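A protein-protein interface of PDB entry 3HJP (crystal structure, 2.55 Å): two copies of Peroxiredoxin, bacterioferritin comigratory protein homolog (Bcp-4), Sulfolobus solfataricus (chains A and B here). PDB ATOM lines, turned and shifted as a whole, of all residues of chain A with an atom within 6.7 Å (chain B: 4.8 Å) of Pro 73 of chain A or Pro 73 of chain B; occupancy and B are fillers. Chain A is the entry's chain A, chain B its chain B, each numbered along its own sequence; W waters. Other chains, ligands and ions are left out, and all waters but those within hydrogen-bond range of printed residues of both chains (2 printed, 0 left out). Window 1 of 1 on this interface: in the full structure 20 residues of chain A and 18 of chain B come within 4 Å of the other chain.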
ATOM      1  N   THR A  16      -2.492  14.813  10.333  1.00  0.00           N
ATOM      2  CA  THR A  16      -3.536  14.670   9.317  1.00  0.00           C
ATOM      3  C   THR A  16      -3.793  13.220   8.926  1.00  0.00           C
ATOM      4  O   THR A  16      -4.895  12.862   8.504  1.00  0.00           O
ATOM      5  CB  THR A  16      -3.191  15.507   8.064  1.00  0.00           C
ATOM      6  OG1 THR A  16      -1.922  15.099   7.532  1.00  0.00           O
ATOM      7  CG2 THR A  16      -3.116  16.986   8.431  1.00  0.00           C
ATOM      8  N   ALA A  39      -7.134  28.941  12.968  1.00  0.00           N
ATOM      9  CA  ALA A  39      -8.022  28.047  12.233  1.00  0.00           C
ATOM     10  C   ALA A  39      -7.718  27.789  10.763  1.00  0.00           C
ATOM     11  O   ALA A  39      -7.251  28.659  10.030  1.00  0.00           O
ATOM     12  CB  ALA A  39      -9.460  28.541  12.368  1.00  0.00           C
ATOM     13  N   SER A  70      -3.255  23.498  15.328  1.00  0.00           N
ATOM     14  CA  SER A  70      -4.498  24.246  15.432  1.00  0.00           C
ATOM     15  C   SER A  70      -5.435  23.293  16.157  1.00  0.00           C
ATOM     16  O   SER A  70      -5.169  22.090  16.212  1.00  0.00           O
ATOM     17  CB  SER A  70      -5.068  24.585  14.043  1.00  0.00           C
ATOM     18  OG  SER A  70      -5.737  23.473  13.465  1.00  0.00           O
ATOM     19  N   VAL A  71      -6.526  23.804  16.715  1.00  0.00           N
ATOM     20  CA  VAL A  71      -7.444  22.920  17.413  1.00  0.00           C
ATOM     21  C   VAL A  71      -8.436  22.262  16.461  1.00  0.00           C
ATOM     22  O   VAL A  71      -9.380  21.588  16.895  1.00  0.00           O
ATOM     23  CB  VAL A  71      -8.199  23.667  18.515  1.00  0.00           C
ATOM     24  CG1 VAL A  71      -7.190  24.267  19.490  1.00  0.00           C
ATOM     25  CG2 VAL A  71      -9.098  24.747  17.909  1.00  0.00           C
ATOM     26  N   ASP A  72      -8.212  22.457  15.163  1.00  0.00           N
ATOM     27  CA  ASP A  72      -9.070  21.889  14.123  1.00  0.00           C
ATOM     28  C   ASP A  72      -8.952  20.370  14.113  1.00  0.00           C
ATOM     29  O   ASP A  72      -7.912  19.833  14.471  1.00  0.00           O
ATOM     30  CB  ASP A  72      -8.659  22.443  12.753  1.00  0.00           C
ATOM     31  CG  ASP A  72      -9.009  23.907  12.591  1.00  0.00           C
ATOM     32  OD1 ASP A  72     -10.212  24.236  12.694  1.00  0.00           O
ATOM     33  OD2 ASP A  72      -8.093  24.726  12.362  1.00  0.00           O
ATOM     34  N   PRO A  73     -10.008  19.661  13.694  1.00  0.00           N
ATOM     35  CA  PRO A  73      -9.968  18.201  13.657  1.00  0.00           C
ATOM     36  C   PRO A  73      -8.948  17.747  12.628  1.00  0.00           C
ATOM     37  O   PRO A  73      -8.580  18.509  11.724  1.00  0.00           O
ATOM     38  CB  PRO A  73     -11.377  17.813  13.212  1.00  0.00           C
ATOM     39  CG  PRO A  73     -12.186  19.045  13.386  1.00  0.00           C
ATOM     40  CD  PRO A  73     -11.238  20.150  13.068  1.00  0.00           C
ATOM     41  N   PRO A  74      -8.470  16.502  12.749  1.00  0.00           N
ATOM     42  CA  PRO A  74      -7.489  16.007  11.773  1.00  0.00           C
ATOM     43  C   PRO A  74      -8.053  15.954  10.345  1.00  0.00           C
ATOM     44  O   PRO A  74      -7.341  16.215   9.374  1.00  0.00           O
ATOM     45  CB  PRO A  74      -7.111  14.619  12.311  1.00  0.00           C
ATOM     46  CG  PRO A  74      -8.254  14.247  13.226  1.00  0.00           C
ATOM     47  CD  PRO A  74      -8.622  15.567  13.872  1.00  0.00           C
ATOM     48  N   PHE A  75      -9.337  15.636  10.227  1.00  0.00           N
ATOM     49  CA  PHE A  75      -9.985  15.547   8.917  1.00  0.00           C
ATOM     50  C   PHE A  75      -9.937  16.860   8.138  1.00  0.00           C
ATOM     51  O   PHE A  75      -9.508  16.892   6.977  1.00  0.00           O
ATOM     52  CB  PHE A  75     -11.434  15.106   9.085  1.00  0.00           C
ATOM     53  CG  PHE A  75     -11.601  13.992  10.065  1.00  0.00           C
ATOM     54  CD1 PHE A  75     -12.158  14.227  11.323  1.00  0.00           C
ATOM     55  CD2 PHE A  75     -11.144  12.706   9.759  1.00  0.00           C
ATOM     56  CE1 PHE A  75     -12.255  13.211  12.259  1.00  0.00           C
ATOM     57  CE2 PHE A  75     -11.238  11.677  10.692  1.00  0.00           C
ATOM     58  CZ  PHE A  75     -11.794  11.932  11.946  1.00  0.00           C
ATOM     59  N   SER A  76     -10.375  17.937   8.781  1.00  0.00           N
ATOM     60  CA  SER A  76     -10.378  19.259   8.170  1.00  0.00           C
ATOM     61  C   SER A  76      -8.956  19.712   7.868  1.00  0.00           C
ATOM     62  O   SER A  76      -8.662  20.203   6.770  1.00  0.00           O
ATOM     63  CB  SER A  76     -11.044  20.276   9.108  1.00  0.00           C
ATOM     64  OG  SER A  76     -12.405  19.955   9.343  1.00  0.00           O
ATOM     65  N   ASN A  77      -8.075  19.556   8.851  1.00  0.00           N
ATOM     66  CA  ASN A  77      -6.678  19.942   8.690  1.00  0.00           C
ATOM     67  C   ASN A  77      -6.045  19.201   7.518  1.00  0.00           C
ATOM     68  O   ASN A  77      -5.178  19.738   6.820  1.00  0.00           O
ATOM     69  CB  ASN A  77      -5.906  19.671   9.986  1.00  0.00           C
ATOM     70  CG  ASN A  77      -5.697  20.929  10.813  1.00  0.00           C
ATOM     71  OD1 ASN A  77      -5.303  20.862  11.982  1.00  0.00           O
ATOM     72  ND2 ASN A  77      -5.942  22.091  10.207  1.00  0.00           N
ATOM     73  N   LYS A  78      -6.477  17.971   7.286  1.00  0.00           N
ATOM     74  CA  LYS A  78      -5.936  17.210   6.173  1.00  0.00           C
ATOM     75  C   LYS A  78      -6.320  17.937   4.885  1.00  0.00           C
ATOM     76  O   LYS A  78      -5.452  18.385   4.133  1.00  0.00           O
ATOM     77  CB  LYS A  78      -6.508  15.798   6.176  1.00  0.00           C
ATOM     78  CG  LYS A  78      -5.877  14.888   5.148  1.00  0.00           C
ATOM     79  CD  LYS A  78      -6.440  13.495   5.254  1.00  0.00           C
ATOM     80  CE  LYS A  78      -5.714  12.565   4.319  1.00  0.00           C
ATOM     81  NZ  LYS A  78      -6.056  11.156   4.655  1.00  0.00           N
ATOM     82  N   SER A  92      -3.433  18.018  15.196  1.00  0.00           N
ATOM     83  CA  SER A  92      -4.713  18.499  15.698  1.00  0.00           C
ATOM     84  C   SER A  92      -4.845  18.513  17.225  1.00  0.00           C
ATOM     85  O   SER A  92      -4.870  17.454  17.875  1.00  0.00           O
ATOM     86  CB  SER A  92      -5.830  17.651  15.087  1.00  0.00           C
ATOM     87  OG  SER A  92      -7.067  17.936  15.698  1.00  0.00           O
ATOM     88  N   ASP A  93      -4.941  19.725  17.777  1.00  0.00           N
ATOM     89  CA  ASP A  93      -5.078  19.934  19.220  1.00  0.00           C
ATOM     90  C   ASP A  93      -6.557  20.026  19.579  1.00  0.00           C
ATOM     91  O   ASP A  93      -6.973  20.923  20.303  1.00  0.00           O
ATOM     92  CB  ASP A  93      -4.357  21.227  19.628  1.00  0.00           C
ATOM     93  CG  ASP A  93      -4.250  21.395  21.144  1.00  0.00           C
ATOM     94  OD1 ASP A  93      -4.195  20.364  21.862  1.00  0.00           O
ATOM     95  OD2 ASP A  93      -4.198  22.560  21.613  1.00  0.00           O
ATOM     96  N   PHE A  94      -7.340  19.068  19.090  1.00  0.00           N
ATOM     97  CA  PHE A  94      -8.772  19.088  19.322  1.00  0.00           C
ATOM     98  C   PHE A  94      -9.261  19.198  20.762  1.00  0.00           C
ATOM     99  O   PHE A  94     -10.428  19.543  20.998  1.00  0.00           O
ATOM    100  CB  PHE A  94      -9.442  17.915  18.594  1.00  0.00           C
ATOM    101  CG  PHE A  94      -9.017  16.565  19.064  1.00  0.00           C
ATOM    102  CD1 PHE A  94      -9.585  15.999  20.200  1.00  0.00           C
ATOM    103  CD2 PHE A  94      -8.106  15.815  18.319  1.00  0.00           C
ATOM    104  CE1 PHE A  94      -9.264  14.704  20.583  1.00  0.00           C
ATOM    105  CE2 PHE A  94      -7.772  14.519  18.689  1.00  0.00           C
ATOM    106  CZ  PHE A  94      -8.351  13.957  19.821  1.00  0.00           C
ATOM    107  N   LEU A 111     -15.302  35.393  17.215  1.00  0.00           N
ATOM    108  CA  LEU A 111     -16.092  34.230  17.644  1.00  0.00           C
ATOM    109  C   LEU A 111     -15.913  33.830  19.111  1.00  0.00           C
ATOM    110  O   LEU A 111     -15.137  32.925  19.426  1.00  0.00           O
ATOM    111  CB  LEU A 111     -15.789  33.028  16.745  1.00  0.00           C
ATOM    112  CG  LEU A 111     -16.589  31.747  17.017  1.00  0.00           C
ATOM    113  CD1 LEU A 111     -18.070  32.080  17.132  1.00  0.00           C
ATOM    114  CD2 LEU A 111     -16.344  30.725  15.893  1.00  0.00           C
ATOM    115  N   TYR A 114     -15.379  30.092  21.441  1.00  0.00           N
ATOM    116  CA  TYR A 114     -14.633  29.083  20.702  1.00  0.00           C
ATOM    117  C   TYR A 114     -13.190  29.209  21.118  1.00  0.00           C
ATOM    118  O   TYR A 114     -12.516  30.146  20.715  1.00  0.00           O
ATOM    119  CB  TYR A 114     -14.747  29.311  19.192  1.00  0.00           C
ATOM    120  CG  TYR A 114     -14.008  28.286  18.348  1.00  0.00           C
ATOM    121  CD1 TYR A 114     -14.459  26.966  18.253  1.00  0.00           C
ATOM    122  CD2 TYR A 114     -12.864  28.644  17.629  1.00  0.00           C
ATOM    123  CE1 TYR A 114     -13.786  26.024  17.460  1.00  0.00           C
ATOM    124  CE2 TYR A 114     -12.181  27.710  16.833  1.00  0.00           C
ATOM    125  CZ  TYR A 114     -12.650  26.404  16.752  1.00  0.00           C
ATOM    126  OH  TYR A 114     -11.990  25.495  15.955  1.00  0.00           O
ATOM    127  N   VAL B  71     -19.598  18.726  14.629  1.00  0.00           N
ATOM    128  CA  VAL B  71     -18.829  19.372  15.681  1.00  0.00           C
ATOM    129  C   VAL B  71     -17.633  20.127  15.109  1.00  0.00           C
ATOM    130  O   VAL B  71     -16.806  20.659  15.869  1.00  0.00           O
ATOM    131  CB  VAL B  71     -18.320  18.342  16.728  1.00  0.00           C
ATOM    132  CG1 VAL B  71     -19.486  17.492  17.218  1.00  0.00           C
ATOM    133  CG2 VAL B  71     -17.207  17.473  16.126  1.00  0.00           C
ATOM    134  N   ASP B  72     -17.542  20.156  13.776  1.00  0.00           N
ATOM    135  CA  ASP B  72     -16.459  20.858  13.069  1.00  0.00           C
ATOM    136  C   ASP B  72     -16.558  22.366  13.313  1.00  0.00           C
ATOM    137  O   ASP B  72     -17.631  22.879  13.623  1.00  0.00           O
ATOM    138  CB  ASP B  72     -16.554  20.609  11.551  1.00  0.00           C
ATOM    139  CG  ASP B  72     -16.189  19.183  11.149  1.00  0.00           C
ATOM    140  OD1 ASP B  72     -15.030  18.770  11.390  1.00  0.00           O
ATOM    141  OD2 ASP B  72     -17.056  18.474  10.588  1.00  0.00           O
ATOM    142  N   PRO B  73     -15.438  23.090  13.185  1.00  0.00           N
ATOM    143  CA  PRO B  73     -15.435  24.543  13.387  1.00  0.00           C
ATOM    144  C   PRO B  73     -16.123  25.221  12.184  1.00  0.00           C
ATOM    145  O   PRO B  73     -16.125  24.693  11.068  1.00  0.00           O
ATOM    146  CB  PRO B  73     -13.947  24.898  13.453  1.00  0.00           C
ATOM    147  CG  PRO B  73     -13.239  23.583  13.606  1.00  0.00           C
ATOM    148  CD  PRO B  73     -14.087  22.611  12.861  1.00  0.00           C
ATOM    149  N   PRO B  74     -16.682  26.415  12.395  1.00  0.00           N
ATOM    150  CA  PRO B  74     -17.377  27.163  11.340  1.00  0.00           C
ATOM    151  C   PRO B  74     -16.531  27.354  10.087  1.00  0.00           C
ATOM    152  O   PRO B  74     -16.987  27.128   8.960  1.00  0.00           O
ATOM    153  CB  PRO B  74     -17.687  28.507  12.005  1.00  0.00           C
ATOM    154  CG  PRO B  74     -17.586  28.231  13.471  1.00  0.00           C
ATOM    155  CD  PRO B  74     -16.460  27.263  13.577  1.00  0.00           C
ATOM    156  N   PHE B  75     -15.294  27.783  10.301  1.00  0.00           N
ATOM    157  CA  PHE B  75     -14.378  28.045   9.208  1.00  0.00           C
ATOM    158  C   PHE B  75     -14.163  26.838   8.294  1.00  0.00           C
ATOM    159  O   PHE B  75     -14.106  26.980   7.069  1.00  0.00           O
ATOM    160  CB  PHE B  75     -13.052  28.551   9.776  1.00  0.00           C
ATOM    161  CG  PHE B  75     -13.229  29.535  10.898  1.00  0.00           C
ATOM    162  CD1 PHE B  75     -13.058  29.136  12.222  1.00  0.00           C
ATOM    163  CD2 PHE B  75     -13.608  30.846  10.638  1.00  0.00           C
ATOM    164  CE1 PHE B  75     -13.258  30.034  13.279  1.00  0.00           C
ATOM    165  CE2 PHE B  75     -13.813  31.746  11.685  1.00  0.00           C
ATOM    166  CZ  PHE B  75     -13.636  31.339  13.009  1.00  0.00           C
ATOM    167  N   SER B  76     -14.059  25.654   8.881  1.00  0.00           N
ATOM    168  CA  SER B  76     -13.865  24.446   8.087  1.00  0.00           C
ATOM    169  C   SER B  76     -15.179  24.048   7.448  1.00  0.00           C
ATOM    170  O   SER B  76     -15.211  23.596   6.302  1.00  0.00           O
ATOM    171  CB  SER B  76     -13.342  23.294   8.960  1.00  0.00           C
ATOM    172  OG  SER B  76     -12.032  23.567   9.435  1.00  0.00           O
ATOM    173  N   ASN B  77     -16.268  24.199   8.186  1.00  0.00           N
ATOM    174  CA  ASN B  77     -17.566  23.842   7.643  1.00  0.00           C
ATOM    175  C   ASN B  77     -17.903  24.779   6.498  1.00  0.00           C
ATOM    176  O   ASN B  77     -18.591  24.388   5.557  1.00  0.00           O
ATOM    177  CB  ASN B  77     -18.639  23.895   8.731  1.00  0.00           C
ATOM    178  CG  ASN B  77     -19.029  22.512   9.223  1.00  0.00           C
ATOM    179  OD1 ASN B  77     -19.626  22.364  10.287  1.00  0.00           O
ATOM    180  ND2 ASN B  77     -18.706  21.495   8.439  1.00  0.00           N
ATOM    181  N   SER B  92     -22.010  24.932  13.246  1.00  0.00           N
ATOM    182  CA  SER B  92     -20.915  24.359  14.030  1.00  0.00           C
ATOM    183  C   SER B  92     -21.261  24.146  15.495  1.00  0.00           C
ATOM    184  O   SER B  92     -21.429  25.105  16.249  1.00  0.00           O
ATOM    185  CB  SER B  92     -19.678  25.250  13.952  1.00  0.00           C
ATOM    186  OG  SER B  92     -19.128  25.213  12.654  1.00  0.00           O
ATOM    187  N   TYR B 114     -11.778  12.065  20.703  1.00  0.00           N
ATOM    188  CA  TYR B 114     -12.439  13.053  19.852  1.00  0.00           C
ATOM    189  C   TYR B 114     -13.936  12.814  19.831  1.00  0.00           C
ATOM    190  O   TYR B 114     -14.416  11.852  19.239  1.00  0.00           O
ATOM    191  CB  TYR B 114     -11.890  12.986  18.422  1.00  0.00           C
ATOM    192  CG  TYR B 114     -12.449  14.050  17.493  1.00  0.00           C
ATOM    193  CD1 TYR B 114     -12.167  15.403  17.701  1.00  0.00           C
ATOM    194  CD2 TYR B 114     -13.295  13.709  16.433  1.00  0.00           C
ATOM    195  CE1 TYR B 114     -12.718  16.392  16.882  1.00  0.00           C
ATOM    196  CE2 TYR B 114     -13.850  14.692  15.614  1.00  0.00           C
ATOM    197  CZ  TYR B 114     -13.557  16.031  15.845  1.00  0.00           C
ATOM    198  OH  TYR B 114     -14.108  17.012  15.041  1.00  0.00           O
HETATM  199  O   HOH W   1     -11.101  25.510  10.623  1.00  0.00           O
HETATM  200  O   HOH W   2     -13.500  17.683   9.638  1.00  0.00           O
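The side-chain carboxylate (OD2) of Asp 72 of chain A is in hydrogen-bond range of the side-chain hydroxyl (OG) of Ser 70 of chain A, 2.9 Å away.
The backbone carbonyl oxygen of Pro 73 of chain B lies close to the side-chain hydroxyl of Ser 92 of chain B (3.4 Å).
OG of Ser 92 of chain A sits at hydrogen-bond distance from O of Asp 72 of chain A (2.4 Å).
N of Pro 74 of chain B lies close to OG of Ser 92 of chain B (2.7 Å).
The side-chain hydroxyl (OG) of Ser 92 of chain B is in hydrogen-bond range of the backbone carbonyl oxygen (O) of Asp 72 of chain B, 2.9 Å away.
CB of Ala 39 of chain A touches CD1 of Phe 75 of chain B (3.6 Å).
Asp 72 of chain A touches Pro 73 of chain B (OD1 to CG, 3.2 Å).
Ser 76 of chain B touches Asp 72 of chain A.
Pro 73 of chain A touches Asp 72 of chain B (CG to OD1, 3.5 Å).
Pro 73 of chain A touches Pro 73 of chain B.
Pro 73 of chain A touches Tyr 114 of chain B (CG to OH, 3.3 Å).
CE1 of Phe 75 of chain A touches CE2 of Tyr 114 of chain B (3.999 Å).
Asp 72 of chain B touches Ser 76 of chain A (OD1 to OG, 3.5 Å).
CD2 of Leu 111 of chain A touches CG of Pro 74 of chain B (3.7 Å).
Pro 73 of chain B touches Tyr 114 of chain A (CB to OH, 3.2 Å).
Printed residues of chain B within 4 Å of Ala 39 of chain A: Phe 75 (3.6 Å).
Of chain B, only Asp 72, Pro 73 and Tyr 114 come within 4 Å of Pro 73 of chain A.
Of chain A, only Asp 72, Pro 73 and Tyr 114 come within 4 Å of Pro 73 of chain B.
Ser 92 of chain B touches none of the printed residues of chain A.
Printed residues of chain A within 4 Å of Tyr 114 of chain B: Pro 73, Phe 75 and Phe 94.
The nearest printed residue of chain B that does not touch Ser 76 of chain A is Pro 73 of chain B (4.7 Å).
Printed residues of chain A that touch a printed residue of chain B: Ala 39, Asp 72, Pro 73, Phe 75, Ser 76, Phe 94, Leu 111 and Tyr 114.
Hydrophobic or aromatic side chains of chain A within 4 Å of the printed part of chain B: Ala 39, Pro 73, Phe 75, Phe 94, Leu 111 and Tyr 114.
Along chain A the printed residues that touch a printed residue of chain B span positions 39 to 114.
Of the 9 printed residues of chain B, 6 touch a printed residue of chain A.
Among the printed residues, 12 pairs touch across the chains.
Among the printed residues, no Asp or Glu carboxylate lies within 4 Å of a Lys or Arg side-chain nitrogen of the other chain.
Asp 72 of chain A touches Pro 73 of chain B, and with the chains exchanged Pro 73 of chain A touches Asp 72 of chain B.
Asp 72 of chain A touches Ser 76 of chain B, and with the chains exchanged Ser 76 of chain A touches Asp 72 of chain B.
Pro 73 of chain B touches its own counterpart, Pro 73 of chain A.
Ser 76 of chain A touches its own counterpart, Ser 76 of chain B.
Positions printed for both chains: 71, 72, 73, 74, 75, 76, 77, 92 and 114.
Water W1 lies within hydrogen-bond range of OG of Ser 76 of chain B and OD1 of Asp 72 of chain A.
Water W2 lies within hydrogen-bond range of the side-chain hydroxyl of Ser 76 of chain A (2.5 Å) and the side-chain carboxylate of Asp 72 of chain B (2.6 Å).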
